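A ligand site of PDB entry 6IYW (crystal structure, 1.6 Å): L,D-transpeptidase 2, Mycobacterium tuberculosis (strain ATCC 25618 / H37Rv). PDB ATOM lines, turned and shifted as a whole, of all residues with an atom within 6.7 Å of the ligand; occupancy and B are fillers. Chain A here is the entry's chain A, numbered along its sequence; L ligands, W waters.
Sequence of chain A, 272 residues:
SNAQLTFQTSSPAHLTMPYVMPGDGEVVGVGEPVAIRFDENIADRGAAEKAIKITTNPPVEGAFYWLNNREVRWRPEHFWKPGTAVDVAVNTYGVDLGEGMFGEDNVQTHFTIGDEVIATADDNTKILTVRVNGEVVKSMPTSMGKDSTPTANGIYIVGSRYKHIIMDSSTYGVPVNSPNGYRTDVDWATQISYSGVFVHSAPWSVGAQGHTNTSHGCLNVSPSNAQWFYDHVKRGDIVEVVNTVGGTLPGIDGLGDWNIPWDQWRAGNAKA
The backbone NH (N) of Cys 218 is in hydrogen-bond range of an oxygen (O1) of the ligand (2.8 Å).
A carbon (C1) of the ligand is bonded to the side-chain sulfur (SG) of Cys 218 (1.8 Å).
An oxygen (O3) of the ligand lies within hydrogen-bond range of the side-chain hydroxyl (OG) of Ser 195 (3.2 Å).
An oxygen (O2) of the ligand lies within hydrogen-bond range of the side-chain sulfur (SD) of Met 167 (3.4 Å).
The backbone carbonyl oxygen (O) of His 216 is in hydrogen-bond range of a nitrogen (N1) of the ligand.
The backbone NH (N) of Gly 217 lies within hydrogen-bond range of an oxygen (O1) of the ligand (3.5 Å).
N of Phe 198 lies within hydrogen-bond range of SG of Cys 218.
The side-chain hydroxyl (OG) of Ser 195 lies within hydrogen-bond range of the side-chain hydroxyl (OG) of Ser 193 (2.7 Å).
N of Ser 195 sits at hydrogen-bond distance from OD1 of Asp 253, at 3.0 Å.
N of Gly 196 lies within hydrogen-bond range of OG of Ser 193.
The backbone carbonyl oxygen (O) of Met 167 is in hydrogen-bond range of the backbone NH (N) of Thr 184 (2.8 Å).
The backbone NH (N) of Gly 217 lies within hydrogen-bond range of the side-chain hydroxyl (OG) of Ser 215, at 2.9 Å.
The backbone carbonyl oxygen (O) of Gly 217 lies within hydrogen-bond range of the side-chain hydroxyl (OG1) of Thr 151 (2.7 Å).
N of Val 197 lies within hydrogen-bond range of OG of Ser 193, 2.9 Å away.
Merely in contact with the ligand: Tyr 182 (3.2 Å), Gly 196 (3.3 Å), Tyr 172 (3.7 Å) and Val 197 (3.7 Å).
Hydrophobic or aromatic side chains that line the ligand: Met 167, Tyr 172, Tyr 182, Val 197 and His 216.
Within 4 Å of the ligand: Met 167, Tyr 172, Tyr 182, Ser 195, Gly 196, Val 197, His 216, Gly 217 and Cys 218.
Along chain A the residues within 4 Å of the ligand span positions 167 to 218.
The nearest printed residue that does not touch the ligand is Ser 215 (4.5 Å).
Water W3 lies within hydrogen-bond range of an oxygen (O2) of the ligand (2.9 Å), a ring nitrogen (NE2) of His 200 (3.0 Å) and the side-chain sulfur (SG) of Cys 218 (3.8 Å).
Water W2 bridges N of His 216 and O1 of the ligand.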
ATOM      1  N   THR A 149     -11.598  -2.175   9.246  1.00  0.00           N
ATOM      2  CA  THR A 149     -12.207  -0.851   9.158  1.00  0.00           C
ATOM      3  C   THR A 149     -13.533  -0.987   8.401  1.00  0.00           C
ATOM      4  O   THR A 149     -13.689  -0.459   7.294  1.00  0.00           O
ATOM      5  CB  THR A 149     -11.301   0.159   8.456  1.00  0.00           C
ATOM      6  OG1 THR A 149     -11.042  -0.291   7.115  1.00  0.00           O
ATOM      7  CG2 THR A 149      -9.974   0.305   9.194  1.00  0.00           C
ATOM      8  N   PRO A 150     -14.500  -1.686   8.985  1.00  0.00           N
ATOM      9  CA  PRO A 150     -15.702  -2.084   8.237  1.00  0.00           C
ATOM     10  C   PRO A 150     -16.710  -0.945   8.075  1.00  0.00           C
ATOM     11  O   PRO A 150     -16.695   0.057   8.792  1.00  0.00           O
ATOM     12  CB  PRO A 150     -16.303  -3.200   9.091  1.00  0.00           C
ATOM     13  CG  PRO A 150     -15.869  -2.848  10.474  1.00  0.00           C
ATOM     14  CD  PRO A 150     -14.510  -2.253  10.347  1.00  0.00           C
ATOM     15  N   THR A 151     -17.595  -1.138   7.087  1.00  0.00           N
ATOM     16  CA  THR A 151     -18.741  -0.258   6.896  1.00  0.00           C
ATOM     17  C   THR A 151     -19.840  -0.628   7.877  1.00  0.00           C
ATOM     18  O   THR A 151     -20.248  -1.784   7.955  1.00  0.00           O
ATOM     19  CB  THR A 151     -19.268  -0.374   5.466  1.00  0.00           C
ATOM     20  OG1 THR A 151     -18.219  -0.089   4.548  1.00  0.00           O
ATOM     21  CG2 THR A 151     -20.388   0.619   5.225  1.00  0.00           C
ATOM     22  N   ALA A 152     -20.350   0.353   8.621  1.00  0.00           N
ATOM     23  CA  ALA A 152     -21.432   0.047   9.557  1.00  0.00           C
ATOM     24  C   ALA A 152     -22.725  -0.292   8.820  1.00  0.00           C
ATOM     25  O   ALA A 152     -23.032   0.282   7.764  1.00  0.00           O
ATOM     26  CB  ALA A 152     -21.678   1.236  10.502  1.00  0.00           C
ATOM     27  N   TYR A 156     -28.756   4.949   5.987  1.00  0.00           N
ATOM     28  CA  TYR A 156     -28.019   6.193   5.761  1.00  0.00           C
ATOM     29  C   TYR A 156     -28.852   7.109   4.885  1.00  0.00           C
ATOM     30  O   TYR A 156     -29.411   6.663   3.882  1.00  0.00           O
ATOM     31  CB  TYR A 156     -26.705   5.901   5.027  1.00  0.00           C
ATOM     32  CG  TYR A 156     -25.648   5.077   5.715  1.00  0.00           C
ATOM     33  CD1 TYR A 156     -25.792   3.712   5.893  1.00  0.00           C
ATOM     34  CD2 TYR A 156     -24.441   5.658   6.069  1.00  0.00           C
ATOM     35  CE1 TYR A 156     -24.768   2.953   6.477  1.00  0.00           C
ATOM     36  CE2 TYR A 156     -23.412   4.922   6.645  1.00  0.00           C
ATOM     37  CZ  TYR A 156     -23.585   3.564   6.846  1.00  0.00           C
ATOM     38  OH  TYR A 156     -22.551   2.836   7.411  1.00  0.00           O
ATOM     39  N   MET A 167      -9.765  13.263   0.379  1.00  0.00           N
ATOM     40  CA  MET A 167      -9.829  12.507   1.621  1.00  0.00           C
ATOM     41  C   MET A 167      -8.460  12.590   2.277  1.00  0.00           C
ATOM     42  O   MET A 167      -7.466  12.103   1.731  1.00  0.00           O
ATOM     43  CB  MET A 167     -10.212  11.060   1.357  1.00  0.00           C
ATOM     44  CG  MET A 167     -11.362  10.897   0.381  1.00  0.00           C
ATOM     45  SD  MET A 167     -12.875  11.616   1.038  1.00  0.00           S
ATOM     46  CE  MET A 167     -14.086  10.737   0.028  1.00  0.00           C
ATOM     47  N   ASP A 168      -8.406  13.204   3.459  1.00  0.00           N
ATOM     48  CA  ASP A 168      -7.140  13.439   4.140  1.00  0.00           C
ATOM     49  C   ASP A 168      -7.269  12.894   5.546  1.00  0.00           C
ATOM     50  O   ASP A 168      -8.087  13.377   6.333  1.00  0.00           O
ATOM     51  CB  ASP A 168      -6.828  14.938   4.158  1.00  0.00           C
ATOM     52  CG  ASP A 168      -5.447  15.244   4.685  1.00  0.00           C
ATOM     53  OD1 ASP A 168      -5.070  14.684   5.741  1.00  0.00           O
ATOM     54  OD2 ASP A 168      -4.740  16.068   4.066  1.00  0.00           O
ATOM     55  N   TYR A 172      -8.928  13.293  10.667  1.00  0.00           N
ATOM     56  CA  TYR A 172      -9.286  12.313  11.693  1.00  0.00           C
ATOM     57  C   TYR A 172      -8.185  12.146  12.734  1.00  0.00           C
ATOM     58  O   TYR A 172      -8.276  11.257  13.590  1.00  0.00           O
ATOM     59  CB  TYR A 172      -9.623  10.975  11.058  1.00  0.00           C
ATOM     60  CG  TYR A 172     -10.821  11.047  10.139  1.00  0.00           C
ATOM     61  CD1 TYR A 172     -10.700  11.496   8.833  1.00  0.00           C
ATOM     62  CD2 TYR A 172     -12.086  10.679  10.596  1.00  0.00           C
ATOM     63  CE1 TYR A 172     -11.801  11.564   7.998  1.00  0.00           C
ATOM     64  CE2 TYR A 172     -13.187  10.747   9.761  1.00  0.00           C
ATOM     65  CZ  TYR A 172     -13.038  11.198   8.467  1.00  0.00           C
ATOM     66  OH  TYR A 172     -14.134  11.277   7.644  1.00  0.00           O
ATOM     67  N   TYR A 182      -3.402   8.684   4.718  1.00  0.00           N
ATOM     68  CA  TYR A 182      -3.774   8.747   3.316  1.00  0.00           C
ATOM     69  C   TYR A 182      -4.116  10.192   2.967  1.00  0.00           C
ATOM     70  O   TYR A 182      -4.490  10.991   3.830  1.00  0.00           O
ATOM     71  CB  TYR A 182      -4.968   7.819   2.991  1.00  0.00           C
ATOM     72  CG  TYR A 182      -6.228   8.091   3.799  1.00  0.00           C
ATOM     73  CD1 TYR A 182      -6.542   7.304   4.895  1.00  0.00           C
ATOM     74  CD2 TYR A 182      -7.076   9.140   3.465  1.00  0.00           C
ATOM     75  CE1 TYR A 182      -7.697   7.553   5.640  1.00  0.00           C
ATOM     76  CE2 TYR A 182      -8.224   9.396   4.209  1.00  0.00           C
ATOM     77  CZ  TYR A 182      -8.528   8.609   5.291  1.00  0.00           C
ATOM     78  OH  TYR A 182      -9.666   8.866   6.021  1.00  0.00           O
ATOM     79  N   THR A 184      -6.023  11.290  -0.553  1.00  0.00           N
ATOM     80  CA  THR A 184      -6.576  10.691  -1.764  1.00  0.00           C
ATOM     81  C   THR A 184      -7.500  11.649  -2.480  1.00  0.00           C
ATOM     82  O   THR A 184      -8.422  12.204  -1.869  1.00  0.00           O
ATOM     83  CB  THR A 184      -7.353   9.409  -1.413  1.00  0.00           C
ATOM     84  OG1 THR A 184      -6.526   8.563  -0.607  1.00  0.00           O
ATOM     85  CG2 THR A 184      -7.788   8.671  -2.652  1.00  0.00           C
ATOM     86  N   VAL A 186     -10.544  11.992  -4.937  1.00  0.00           N
ATOM     87  CA  VAL A 186     -11.681  11.118  -5.195  1.00  0.00           C
ATOM     88  C   VAL A 186     -12.691  11.840  -6.072  1.00  0.00           C
ATOM     89  O   VAL A 186     -13.033  13.003  -5.790  1.00  0.00           O
ATOM     90  CB  VAL A 186     -12.316  10.663  -3.873  1.00  0.00           C
ATOM     91  CG1 VAL A 186     -13.707  10.162  -4.103  1.00  0.00           C
ATOM     92  CG2 VAL A 186     -11.435   9.609  -3.196  1.00  0.00           C
ATOM     93  N   SER A 193     -22.684   9.628   5.372  1.00  0.00           N
ATOM     94  CA  SER A 193     -22.645   9.864   6.824  1.00  0.00           C
ATOM     95  C   SER A 193     -21.755  11.057   7.117  1.00  0.00           C
ATOM     96  O   SER A 193     -20.791  11.324   6.408  1.00  0.00           O
ATOM     97  CB  SER A 193     -22.123   8.660   7.616  1.00  0.00           C
ATOM     98  OG  SER A 193     -20.700   8.502   7.456  1.00  0.00           O
ATOM     99  N   TYR A 194     -22.076  11.776   8.203  1.00  0.00           N
ATOM    100  CA  TYR A 194     -21.199  12.847   8.669  1.00  0.00           C
ATOM    101  C   TYR A 194     -19.844  12.292   9.095  1.00  0.00           C
ATOM    102  O   TYR A 194     -18.826  13.012   9.026  1.00  0.00           O
ATOM    103  CB  TYR A 194     -21.806  13.634   9.847  1.00  0.00           C
ATOM    104  CG  TYR A 194     -22.881  14.648   9.497  1.00  0.00           C
ATOM    105  CD1 TYR A 194     -23.622  14.549   8.329  1.00  0.00           C
ATOM    106  CD2 TYR A 194     -23.168  15.688  10.371  1.00  0.00           C
ATOM    107  CE1 TYR A 194     -24.616  15.449   8.035  1.00  0.00           C
ATOM    108  CE2 TYR A 194     -24.163  16.607  10.092  1.00  0.00           C
ATOM    109  CZ  TYR A 194     -24.887  16.486   8.913  1.00  0.00           C
ATOM    110  OH  TYR A 194     -25.886  17.394   8.623  1.00  0.00           O
ATOM    111  N   SER A 195     -19.811  11.060   9.597  1.00  0.00           N
ATOM    112  CA  SER A 195     -18.571  10.442  10.050  1.00  0.00           C
ATOM    113  C   SER A 195     -17.595  10.248   8.903  1.00  0.00           C
ATOM    114  O   SER A 195     -16.403  10.091   9.147  1.00  0.00           O
ATOM    115  CB  SER A 195     -18.842   9.100  10.730  1.00  0.00           C
ATOM    116  OG  SER A 195     -19.404   8.142   9.845  1.00  0.00           O
ATOM    117  N   GLY A 196     -18.083  10.245   7.668  1.00  0.00           N
ATOM    118  CA  GLY A 196     -17.199  10.264   6.523  1.00  0.00           C
ATOM    119  C   GLY A 196     -17.410   9.168   5.487  1.00  0.00           C
ATOM    120  O   GLY A 196     -16.551   9.006   4.614  1.00  0.00           O
ATOM    121  N   VAL A 197     -18.499   8.410   5.572  1.00  0.00           N
ATOM    122  CA  VAL A 197     -18.810   7.402   4.556  1.00  0.00           C
ATOM    123  C   VAL A 197     -19.338   8.086   3.309  1.00  0.00           C
ATOM    124  O   VAL A 197     -20.277   8.881   3.374  1.00  0.00           O
ATOM    125  CB  VAL A 197     -19.811   6.363   5.080  1.00  0.00           C
ATOM    126  CG1 VAL A 197     -20.100   5.318   4.006  1.00  0.00           C
ATOM    127  CG2 VAL A 197     -19.312   5.686   6.349  1.00  0.00           C
ATOM    128  N   PHE A 198     -18.761   7.752   2.163  1.00  0.00           N
ATOM    129  CA  PHE A 198     -19.193   8.205   0.844  1.00  0.00           C
ATOM    130  C   PHE A 198     -19.379   6.997  -0.063  1.00  0.00           C
ATOM    131  O   PHE A 198     -18.700   5.971   0.086  1.00  0.00           O
ATOM    132  CB  PHE A 198     -18.143   9.103   0.187  1.00  0.00           C
ATOM    133  CG  PHE A 198     -18.034  10.451   0.795  1.00  0.00           C
ATOM    134  CD1 PHE A 198     -17.350  10.634   1.979  1.00  0.00           C
ATOM    135  CD2 PHE A 198     -18.537  11.551   0.136  1.00  0.00           C
ATOM    136  CE1 PHE A 198     -17.207  11.906   2.548  1.00  0.00           C
ATOM    137  CE2 PHE A 198     -18.406  12.834   0.690  1.00  0.00           C
ATOM    138  CZ  PHE A 198     -17.728  12.998   1.904  1.00  0.00           C
ATOM    139  N   HIS A 200     -18.353   6.468  -3.826  1.00  0.00           N
ATOM    140  CA  HIS A 200     -17.498   7.260  -4.697  1.00  0.00           C
ATOM    141  C   HIS A 200     -16.750   6.378  -5.675  1.00  0.00           C
ATOM    142  O   HIS A 200     -16.743   5.151  -5.562  1.00  0.00           O
ATOM    143  CB  HIS A 200     -16.516   8.118  -3.903  1.00  0.00           C
ATOM    144  CG  HIS A 200     -15.480   7.343  -3.154  1.00  0.00           C
ATOM    145  ND1 HIS A 200     -14.343   6.849  -3.762  1.00  0.00           N
ATOM    146  CD2 HIS A 200     -15.404   6.972  -1.856  1.00  0.00           C
ATOM    147  CE1 HIS A 200     -13.614   6.209  -2.867  1.00  0.00           C
ATOM    148  NE2 HIS A 200     -14.231   6.269  -1.701  1.00  0.00           N
ATOM    149  N   SER A 215     -11.896  -1.144   1.439  1.00  0.00           N
ATOM    150  CA  SER A 215     -11.874   0.288   1.707  1.00  0.00           C
ATOM    151  C   SER A 215     -11.721   0.583   3.196  1.00  0.00           C
ATOM    152  O   SER A 215     -11.718  -0.307   4.041  1.00  0.00           O
ATOM    153  CB  SER A 215     -13.147   0.945   1.176  1.00  0.00           C
ATOM    154  OG  SER A 215     -14.208   0.816   2.121  1.00  0.00           O
ATOM    155  N   HIS A 216     -11.624   1.880   3.527  1.00  0.00           N
ATOM    156  CA  HIS A 216     -11.621   2.357   4.903  1.00  0.00           C
ATOM    157  C   HIS A 216     -13.017   2.487   5.501  1.00  0.00           C
ATOM    158  O   HIS A 216     -13.140   2.972   6.630  1.00  0.00           O
ATOM    159  CB  HIS A 216     -10.919   3.715   5.005  1.00  0.00           C
ATOM    160  CG  HIS A 216      -9.487   3.701   4.592  1.00  0.00           C
ATOM    161  ND1 HIS A 216      -8.473   3.323   5.445  1.00  0.00           N
ATOM    162  CD2 HIS A 216      -8.889   4.027   3.418  1.00  0.00           C
ATOM    163  CE1 HIS A 216      -7.317   3.415   4.815  1.00  0.00           C
ATOM    164  NE2 HIS A 216      -7.542   3.829   3.578  1.00  0.00           N
ATOM    165  N   GLY A 217     -14.053   2.072   4.777  1.00  0.00           N
ATOM    166  CA  GLY A 217     -15.431   2.247   5.228  1.00  0.00           C
ATOM    167  C   GLY A 217     -16.338   2.730   4.112  1.00  0.00           C
ATOM    168  O   GLY A 217     -17.542   2.455   4.114  1.00  0.00           O
ATOM    169  N   CYS A 218     -15.752   3.413   3.138  1.00  0.00           N
ATOM    170  CA  CYS A 218     -16.517   3.964   2.031  1.00  0.00           C
ATOM    171  C   CYS A 218     -17.036   2.861   1.121  1.00  0.00           C
ATOM    172  O   CYS A 218     -16.535   1.734   1.105  1.00  0.00           O
ATOM    173  CB  CYS A 218     -15.651   4.927   1.246  1.00  0.00           C
ATOM    174  SG  CYS A 218     -15.437   6.486   2.154  1.00  0.00           S
ATOM    175  N   LEU A 219     -18.060   3.201   0.329  1.00  0.00           N
ATOM    176  CA  LEU A 219     -18.626   2.275  -0.656  1.00  0.00           C
ATOM    177  C   LEU A 219     -17.959   2.570  -1.991  1.00  0.00           C
ATOM    178  O   LEU A 219     -18.362   3.500  -2.699  1.00  0.00           O
ATOM    179  CB  LEU A 219     -20.145   2.408  -0.739  1.00  0.00           C
ATOM    180  CG  LEU A 219     -20.911   1.642   0.334  1.00  0.00           C
ATOM    181  CD1 LEU A 219     -20.578   2.128   1.727  1.00  0.00           C
ATOM    182  CD2 LEU A 219     -22.392   1.792   0.081  1.00  0.00           C
ATOM    183  N   ASN A 220     -16.899   1.803  -2.307  1.00  0.00           N
ATOM    184  CA  ASN A 220     -16.179   1.943  -3.574  1.00  0.00           C
ATOM    185  C   ASN A 220     -16.991   1.363  -4.713  1.00  0.00           C
ATOM    186  O   ASN A 220     -17.387   0.192  -4.643  1.00  0.00           O
ATOM    187  CB  ASN A 220     -14.848   1.168  -3.575  1.00  0.00           C
ATOM    188  CG  ASN A 220     -13.744   1.772  -2.737  1.00  0.00           C
ATOM    189  OD1 ASN A 220     -12.626   1.238  -2.764  1.00  0.00           O
ATOM    190  ND2 ASN A 220     -14.004   2.859  -2.025  1.00  0.00           N
ATOM    191  N   ASP A 253     -25.476  10.399  14.150  1.00  0.00           N
ATOM    192  CA  ASP A 253     -24.367  10.710  13.250  1.00  0.00           C
ATOM    193  C   ASP A 253     -24.526  12.054  12.567  1.00  0.00           C
ATOM    194  O   ASP A 253     -23.543  12.796  12.396  1.00  0.00           O
ATOM    195  CB  ASP A 253     -24.250   9.631  12.179  1.00  0.00           C
ATOM    196  CG  ASP A 253     -23.426  10.077  10.985  1.00  0.00           C
ATOM    197  OD1 ASP A 253     -22.197   9.876  11.045  1.00  0.00           O
ATOM    198  OD2 ASP A 253     -23.977  10.604   9.993  1.00  0.00           O
HETATM  199  C1  LIG L   1     -14.146   6.178   3.369  1.00  0.00           C
HETATM  200  C2  LIG L   1     -13.919   7.389   7.912  1.00  0.00           C
HETATM  201  C3  LIG L   1     -13.768   7.327   4.402  1.00  0.00           C
HETATM  202  C4  LIG L   1     -13.502   6.750   5.676  1.00  0.00           C
HETATM  203  C5  LIG L   1     -14.928   6.389   7.421  1.00  0.00           C
HETATM  204  O1  LIG L   1     -13.544   5.152   3.285  1.00  0.00           O
HETATM  205  C6  LIG L   1     -12.531   8.124   3.863  1.00  0.00           C
HETATM  206  O2  LIG L   1     -12.820   8.589   2.584  1.00  0.00           O
HETATM  207  C7  LIG L   1     -11.309   7.228   3.766  1.00  0.00           C
HETATM  208  N1  LIG L   1     -14.777   5.957   6.175  1.00  0.00           N
HETATM  209  C8  LIG L   1     -16.060   5.891   8.333  1.00  0.00           C
HETATM  210  O3  LIG L   1     -16.713   6.692   9.044  1.00  0.00           O
HETATM  211  O4  LIG L   1     -16.346   4.663   8.363  1.00  0.00           O
HETATM  212  S1  LIG L   1     -12.962   6.931   9.394  1.00  0.00           S
HETATM  213  C9  LIG L   1     -11.865   5.544   9.008  1.00  0.00           C
HETATM  214  C10 LIG L   1     -13.229   7.833   6.786  1.00  0.00           C
HETATM  215  O   HOH W   1     -11.262  11.124   4.855  1.00  0.00           O
HETATM  216  O   HOH W   2     -11.549   3.931   0.972  1.00  0.00           O
HETATM  217  O   HOH W   3     -12.122   6.813   0.417  1.00  0.00           O
HETATM  218  O   HOH W   4     -14.822   2.178   9.094  1.00  0.00           O
